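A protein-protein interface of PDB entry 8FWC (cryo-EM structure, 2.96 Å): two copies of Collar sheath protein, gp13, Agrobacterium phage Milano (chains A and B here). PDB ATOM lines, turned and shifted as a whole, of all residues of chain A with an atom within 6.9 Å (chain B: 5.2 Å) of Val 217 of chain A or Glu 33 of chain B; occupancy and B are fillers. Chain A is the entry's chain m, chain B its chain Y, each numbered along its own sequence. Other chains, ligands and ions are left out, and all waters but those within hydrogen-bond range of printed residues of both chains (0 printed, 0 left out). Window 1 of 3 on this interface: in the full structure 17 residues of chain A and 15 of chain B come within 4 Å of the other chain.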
ATOM      1  N   ASP A   7       8.352 -13.130 -16.252  1.00  0.00           N
ATOM      2  CA  ASP A   7       8.088 -14.156 -17.248  1.00  0.00           C
ATOM      3  C   ASP A   7       7.379 -15.340 -16.601  1.00  0.00           C
ATOM      4  O   ASP A   7       7.753 -15.769 -15.510  1.00  0.00           O
ATOM      5  CB  ASP A   7       9.377 -14.600 -17.949  1.00  0.00           C
ATOM      6  CG  ASP A   7       9.992 -15.852 -17.351  1.00  0.00           C
ATOM      7  OD1 ASP A   7      10.459 -15.784 -16.194  1.00  0.00           O
ATOM      8  OD2 ASP A   7       9.989 -16.901 -18.031  1.00  0.00           O
ATOM      9  N   ARG A   9       6.854 -18.623 -16.859  1.00  0.00           N
ATOM     10  CA  ARG A   9       7.278 -20.019 -16.730  1.00  0.00           C
ATOM     11  C   ARG A   9       6.247 -20.977 -17.326  1.00  0.00           C
ATOM     12  O   ARG A   9       5.759 -21.895 -16.668  1.00  0.00           O
ATOM     13  CB  ARG A   9       7.561 -20.374 -15.275  1.00  0.00           C
ATOM     14  CG  ARG A   9       8.288 -19.301 -14.499  1.00  0.00           C
ATOM     15  CD  ARG A   9       9.620 -18.979 -15.105  1.00  0.00           C
ATOM     16  NE  ARG A   9      10.462 -20.157 -15.231  1.00  0.00           N
ATOM     17  CZ  ARG A   9      11.494 -20.223 -16.057  1.00  0.00           C
ATOM     18  NH1 ARG A   9      11.781 -19.179 -16.816  1.00  0.00           N
ATOM     19  NH2 ARG A   9      12.230 -21.319 -16.135  1.00  0.00           N
ATOM     20  N   TRP A  44       2.607 -15.148 -13.410  1.00  0.00           N
ATOM     21  CA  TRP A  44       3.138 -16.395 -12.878  1.00  0.00           C
ATOM     22  C   TRP A  44       2.317 -16.942 -11.726  1.00  0.00           C
ATOM     23  O   TRP A  44       2.095 -18.152 -11.653  1.00  0.00           O
ATOM     24  CB  TRP A  44       4.581 -16.195 -12.413  1.00  0.00           C
ATOM     25  CG  TRP A  44       5.156 -17.330 -11.625  1.00  0.00           C
ATOM     26  CD1 TRP A  44       5.568 -18.530 -12.105  1.00  0.00           C
ATOM     27  CD2 TRP A  44       5.406 -17.355 -10.220  1.00  0.00           C
ATOM     28  NE1 TRP A  44       6.050 -19.307 -11.087  1.00  0.00           N
ATOM     29  CE2 TRP A  44       5.959 -18.605  -9.918  1.00  0.00           C
ATOM     30  CE3 TRP A  44       5.208 -16.442  -9.187  1.00  0.00           C
ATOM     31  CZ2 TRP A  44       6.315 -18.963  -8.632  1.00  0.00           C
ATOM     32  CZ3 TRP A  44       5.564 -16.800  -7.916  1.00  0.00           C
ATOM     33  CH2 TRP A  44       6.110 -18.046  -7.646  1.00  0.00           C
ATOM     34  N   ARG A 205      14.260 -13.043  -5.110  1.00  0.00           N
ATOM     35  CA  ARG A 205      13.685 -14.361  -4.883  1.00  0.00           C
ATOM     36  C   ARG A 205      12.354 -14.198  -4.171  1.00  0.00           C
ATOM     37  O   ARG A 205      12.321 -13.897  -2.976  1.00  0.00           O
ATOM     38  CB  ARG A 205      14.621 -15.237  -4.059  1.00  0.00           C
ATOM     39  CG  ARG A 205      14.017 -16.555  -3.639  1.00  0.00           C
ATOM     40  CD  ARG A 205      14.943 -17.297  -2.709  1.00  0.00           C
ATOM     41  NE  ARG A 205      14.479 -18.645  -2.418  1.00  0.00           N
ATOM     42  CZ  ARG A 205      13.618 -18.942  -1.456  1.00  0.00           C
ATOM     43  NH1 ARG A 205      13.125 -17.983  -0.694  1.00  0.00           N
ATOM     44  NH2 ARG A 205      13.251 -20.197  -1.255  1.00  0.00           N
ATOM     45  N   GLN A 206      11.267 -14.418  -4.893  1.00  0.00           N
ATOM     46  CA  GLN A 206       9.927 -14.177  -4.391  1.00  0.00           C
ATOM     47  C   GLN A 206       9.178 -15.493  -4.277  1.00  0.00           C
ATOM     48  O   GLN A 206       9.233 -16.322  -5.184  1.00  0.00           O
ATOM     49  CB  GLN A 206       9.177 -13.227  -5.312  1.00  0.00           C
ATOM     50  CG  GLN A 206       7.707 -13.162  -5.060  1.00  0.00           C
ATOM     51  CD  GLN A 206       7.374 -12.445  -3.784  1.00  0.00           C
ATOM     52  OE1 GLN A 206       7.546 -12.974  -2.694  1.00  0.00           O
ATOM     53  NE2 GLN A 206       6.893 -11.227  -3.912  1.00  0.00           N
ATOM     54  N   VAL A 207       8.463 -15.674  -3.171  1.00  0.00           N
ATOM     55  CA  VAL A 207       7.720 -16.897  -2.903  1.00  0.00           C
ATOM     56  C   VAL A 207       6.238 -16.603  -3.025  1.00  0.00           C
ATOM     57  O   VAL A 207       5.735 -15.658  -2.411  1.00  0.00           O
ATOM     58  CB  VAL A 207       8.021 -17.458  -1.506  1.00  0.00           C
ATOM     59  CG1 VAL A 207       9.087 -18.498  -1.583  1.00  0.00           C
ATOM     60  CG2 VAL A 207       8.464 -16.359  -0.614  1.00  0.00           C
ATOM     61  N   ALA A 208       5.545 -17.411  -3.803  1.00  0.00           N
ATOM     62  CA  ALA A 208       4.101 -17.470  -3.746  1.00  0.00           C
ATOM     63  C   ALA A 208       3.740 -18.510  -2.701  1.00  0.00           C
ATOM     64  O   ALA A 208       4.600 -19.003  -1.970  1.00  0.00           O
ATOM     65  CB  ALA A 208       3.517 -17.793  -5.118  1.00  0.00           C
ATOM     66  N   GLU A 215       4.966 -23.748  -0.778  1.00  0.00           N
ATOM     67  CA  GLU A 215       5.741 -22.643  -1.320  1.00  0.00           C
ATOM     68  C   GLU A 215       5.993 -22.833  -2.805  1.00  0.00           C
ATOM     69  O   GLU A 215       6.172 -23.954  -3.281  1.00  0.00           O
ATOM     70  CB  GLU A 215       7.070 -22.509  -0.585  1.00  0.00           C
ATOM     71  CG  GLU A 215       7.007 -21.599   0.613  1.00  0.00           C
ATOM     72  CD  GLU A 215       8.367 -21.133   1.055  1.00  0.00           C
ATOM     73  OE1 GLU A 215       9.372 -21.572   0.461  1.00  0.00           O
ATOM     74  OE2 GLU A 215       8.437 -20.362   2.028  1.00  0.00           O
ATOM     75  N   PHE A 216       6.027 -21.713  -3.520  1.00  0.00           N
ATOM     76  CA  PHE A 216       6.412 -21.668  -4.923  1.00  0.00           C
ATOM     77  C   PHE A 216       7.417 -20.543  -5.083  1.00  0.00           C
ATOM     78  O   PHE A 216       7.060 -19.376  -4.919  1.00  0.00           O
ATOM     79  CB  PHE A 216       5.209 -21.415  -5.828  1.00  0.00           C
ATOM     80  CG  PHE A 216       4.281 -22.574  -5.961  1.00  0.00           C
ATOM     81  CD1 PHE A 216       4.575 -23.612  -6.807  1.00  0.00           C
ATOM     82  CD2 PHE A 216       3.089 -22.602  -5.277  1.00  0.00           C
ATOM     83  CE1 PHE A 216       3.715 -24.666  -6.947  1.00  0.00           C
ATOM     84  CE2 PHE A 216       2.229 -23.655  -5.416  1.00  0.00           C
ATOM     85  CZ  PHE A 216       2.543 -24.686  -6.251  1.00  0.00           C
ATOM     86  N   VAL A 217       8.649 -20.875  -5.407  1.00  0.00           N
ATOM     87  CA  VAL A 217       9.724 -19.898  -5.485  1.00  0.00           C
ATOM     88  C   VAL A 217       9.886 -19.424  -6.920  1.00  0.00           C
ATOM     89  O   VAL A 217       9.594 -20.148  -7.875  1.00  0.00           O
ATOM     90  CB  VAL A 217      11.031 -20.502  -4.943  1.00  0.00           C
ATOM     91  CG1 VAL A 217      12.046 -19.426  -4.695  1.00  0.00           C
ATOM     92  CG2 VAL A 217      10.746 -21.259  -3.677  1.00  0.00           C
ATOM     93  N   HIS A 218      10.347 -18.186  -7.071  1.00  0.00           N
ATOM     94  CA  HIS A 218      10.559 -17.558  -8.364  1.00  0.00           C
ATOM     95  C   HIS A 218      11.769 -16.646  -8.268  1.00  0.00           C
ATOM     96  O   HIS A 218      11.867 -15.848  -7.336  1.00  0.00           O
ATOM     97  CB  HIS A 218       9.339 -16.751  -8.790  1.00  0.00           C
ATOM     98  CG  HIS A 218       9.435 -16.195 -10.173  1.00  0.00           C
ATOM     99  ND1 HIS A 218      10.410 -15.302 -10.547  1.00  0.00           N
ATOM    100  CD2 HIS A 218       8.671 -16.399 -11.269  1.00  0.00           C
ATOM    101  CE1 HIS A 218      10.254 -14.992 -11.819  1.00  0.00           C
ATOM    102  NE2 HIS A 218       9.200 -15.638 -12.279  1.00  0.00           N
ATOM    103  N   ILE A 219      12.688 -16.754  -9.224  1.00  0.00           N
ATOM    104  CA  ILE A 219      13.933 -15.997  -9.195  1.00  0.00           C
ATOM    105  C   ILE A 219      14.100 -15.243 -10.506  1.00  0.00           C
ATOM    106  O   ILE A 219      13.845 -15.795 -11.579  1.00  0.00           O
ATOM    107  CB  ILE A 219      15.147 -16.906  -8.949  1.00  0.00           C
ATOM    108  CG1 ILE A 219      14.917 -17.775  -7.721  1.00  0.00           C
ATOM    109  CG2 ILE A 219      16.390 -16.076  -8.761  1.00  0.00           C
ATOM    110  CD1 ILE A 219      16.161 -18.428  -7.211  1.00  0.00           C
ATOM    111  N   ALA B  29      13.739 -25.431 -16.612  1.00  0.00           N
ATOM    112  CA  ALA B  29      13.811 -25.218 -15.177  1.00  0.00           C
ATOM    113  C   ALA B  29      15.056 -24.414 -14.846  1.00  0.00           C
ATOM    114  O   ALA B  29      16.069 -24.503 -15.539  1.00  0.00           O
ATOM    115  CB  ALA B  29      13.823 -26.545 -14.422  1.00  0.00           C
ATOM    116  N   ARG B  30      14.966 -23.628 -13.778  1.00  0.00           N
ATOM    117  CA  ARG B  30      16.032 -22.754 -13.332  1.00  0.00           C
ATOM    118  C   ARG B  30      16.440 -23.107 -11.909  1.00  0.00           C
ATOM    119  O   ARG B  30      15.574 -23.319 -11.059  1.00  0.00           O
ATOM    120  CB  ARG B  30      15.587 -21.291 -13.396  1.00  0.00           C
ATOM    121  CG  ARG B  30      16.380 -20.362 -12.514  1.00  0.00           C
ATOM    122  CD  ARG B  30      16.230 -18.923 -12.950  1.00  0.00           C
ATOM    123  NE  ARG B  30      17.319 -18.099 -12.441  1.00  0.00           N
ATOM    124  CZ  ARG B  30      17.572 -16.862 -12.851  1.00  0.00           C
ATOM    125  NH1 ARG B  30      16.811 -16.300 -13.777  1.00  0.00           N
ATOM    126  NH2 ARG B  30      18.587 -16.186 -12.335  1.00  0.00           N
ATOM    127  N   PRO B  31      17.737 -23.184 -11.618  1.00  0.00           N
ATOM    128  CA  PRO B  31      18.172 -23.639 -10.293  1.00  0.00           C
ATOM    129  C   PRO B  31      17.668 -22.765  -9.162  1.00  0.00           C
ATOM    130  O   PRO B  31      17.902 -21.556  -9.150  1.00  0.00           O
ATOM    131  CB  PRO B  31      19.699 -23.584 -10.392  1.00  0.00           C
ATOM    132  CG  PRO B  31      19.983 -23.642 -11.829  1.00  0.00           C
ATOM    133  CD  PRO B  31      18.878 -22.911 -12.498  1.00  0.00           C
ATOM    134  N   GLY B  32      16.974 -23.369  -8.206  1.00  0.00           N
ATOM    135  CA  GLY B  32      16.421 -22.667  -7.068  1.00  0.00           C
ATOM    136  C   GLY B  32      14.920 -22.505  -7.115  1.00  0.00           C
ATOM    137  O   GLY B  32      14.295 -22.321  -6.064  1.00  0.00           O
ATOM    138  N   GLU B  33      14.322 -22.571  -8.298  1.00  0.00           N
ATOM    139  CA  GLU B  33      12.892 -22.392  -8.451  1.00  0.00           C
ATOM    140  C   GLU B  33      12.115 -23.537  -7.819  1.00  0.00           C
ATOM    141  O   GLU B  33      12.656 -24.594  -7.501  1.00  0.00           O
ATOM    142  CB  GLU B  33      12.520 -22.315  -9.923  1.00  0.00           C
ATOM    143  CG  GLU B  33      12.322 -20.929 -10.450  1.00  0.00           C
ATOM    144  CD  GLU B  33      11.660 -20.943 -11.803  1.00  0.00           C
ATOM    145  OE1 GLU B  33      11.497 -22.047 -12.366  1.00  0.00           O
ATOM    146  OE2 GLU B  33      11.302 -19.858 -12.304  1.00  0.00           O
ATOM    147  N   VAL B  34      10.819 -23.302  -7.640  1.00  0.00           N
ATOM    148  CA  VAL B  34       9.841 -24.331  -7.314  1.00  0.00           C
ATOM    149  C   VAL B  34       8.586 -23.968  -8.090  1.00  0.00           C
ATOM    150  O   VAL B  34       7.873 -23.035  -7.713  1.00  0.00           O
ATOM    151  CB  VAL B  34       9.539 -24.415  -5.813  1.00  0.00           C
ATOM    152  CG1 VAL B  34       8.422 -25.375  -5.573  1.00  0.00           C
ATOM    153  CG2 VAL B  34      10.755 -24.852  -5.045  1.00  0.00           C
ATOM    154  N   ASN B  35       8.320 -24.681  -9.170  1.00  0.00           N
ATOM    155  CA  ASN B  35       7.248 -24.321 -10.079  1.00  0.00           C
ATOM    156  C   ASN B  35       6.063 -25.269  -9.888  1.00  0.00           C
ATOM    157  O   ASN B  35       6.080 -26.135  -9.013  1.00  0.00           O
ATOM    158  CB  ASN B  35       7.792 -24.331 -11.506  1.00  0.00           C
ATOM    159  CG  ASN B  35       6.962 -23.504 -12.443  1.00  0.00           C
ATOM    160  OD1 ASN B  35       5.947 -22.941 -12.051  1.00  0.00           O
ATOM    161  ND2 ASN B  35       7.384 -23.425 -13.693  1.00  0.00           N
ATOM    162  N   LEU B 188       7.145 -29.175  -8.982  1.00  0.00           N
ATOM    163  CA  LEU B 188       8.450 -29.587  -9.483  1.00  0.00           C
ATOM    164  C   LEU B 188       9.485 -28.596  -8.975  1.00  0.00           C
ATOM    165  O   LEU B 188       9.483 -27.435  -9.385  1.00  0.00           O
ATOM    166  CB  LEU B 188       8.459 -29.647 -11.005  1.00  0.00           C
ATOM    167  CG  LEU B 188       9.828 -29.840 -11.642  1.00  0.00           C
ATOM    168  CD1 LEU B 188      10.166 -31.307 -11.695  1.00  0.00           C
ATOM    169  CD2 LEU B 188       9.843 -29.237 -13.021  1.00  0.00           C
ATOM    170  N   GLY B 189      10.368 -29.051  -8.105  1.00  0.00           N
ATOM    171  CA  GLY B 189      11.359 -28.188  -7.483  1.00  0.00           C
ATOM    172  C   GLY B 189      12.755 -28.523  -7.967  1.00  0.00           C
ATOM    173  O   GLY B 189      13.082 -29.688  -8.172  1.00  0.00           O
ATOM    174  N   VAL B 190      13.570 -27.490  -8.146  1.00  0.00           N
ATOM    175  CA  VAL B 190      14.937 -27.621  -8.629  1.00  0.00           C
ATOM    176  C   VAL B 190      15.872 -27.118  -7.543  1.00  0.00           C
ATOM    177  O   VAL B 190      15.732 -25.984  -7.075  1.00  0.00           O
ATOM    178  CB  VAL B 190      15.148 -26.841  -9.931  1.00  0.00           C
ATOM    179  CG1 VAL B 190      16.469 -27.202 -10.541  1.00  0.00           C
ATOM    180  CG2 VAL B 190      14.026 -27.120 -10.893  1.00  0.00           C
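N of Val 217 of chain A lies within hydrogen-bond range of O of Val 34 of chain B (3.3 Å).
OE2 of Glu 33 of chain B is in salt-bridge range of NE of Arg 9 of chain A, at 3.1 Å.
Of the printed residues of chain B, Arg 9 of chain A touches Glu 33 and Asn 35.
His 218 of chain A touches none of the printed residues of chain B.
Gly 32 of chain B touches just one residue of chain A: Val 217.
Of chain A, only Arg 9 and Val 217 come within 4 Å of Glu 33 of chain B.
Of the printed residues of chain A, Asn 35 of chain B touches Arg 9, Trp 44 and Phe 216.
The nearest printed residue of chain A that does not touch Arg 30 of chain B is Arg 9 of chain A (4.3 Å).
Asn 35 of chain B touches Arg 9 of chain A (ND2 to CB, 3.4 Å).
Trp 44 of chain A touches Asn 35 of chain B.
CG1 of Val 34 of chain B touches O of Glu 215 of chain A, 3.5 Å away.
Phe 216 of chain A touches Val 34 of chain B (CA to O, 3.4 Å).
CE1 of Phe 216 of chain A touches O of Asn 35 of chain B (3.5 Å).
Gly 32 of chain B touches Val 217 of chain A.
CG of Glu 33 of chain B touches O of Val 217 of chain A (3.8 Å).
NH1 of Arg 30 of chain B touches O of Ile 219 of chain A, 3.7 Å away.
O of Glu 33 of chain B is in hydrogen-bond range of N of Val 190 of chain B (3.1 Å).
N of Gly 32 of chain B is in hydrogen-bond range of O of Val 190 of chain B.
The backbone carbonyl oxygen (O) of Leu 188 of chain B sits at hydrogen-bond distance from the backbone NH (N) of Asn 35 of chain B (3.0 Å).
The backbone NH of Ala 208 of chain A is in hydrogen-bond range of the backbone carbonyl oxygen of Phe 216 of chain A (2.7 Å).
The side-chain carboxylate of Asp 7 of chain A lies within salt-bridge range of the guanidinium group of Arg 9 of chain A (3.1 Å).
Of the 10 printed residues of chain B, 5 touch a printed residue of chain A.
Printed residues of chain B that touch a printed residue of chain A: Arg 30, Gly 32, Glu 33, Val 34 and Asn 35.
Among the printed residues, 10 pairs touch across the chains.
No position is printed for both chains.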
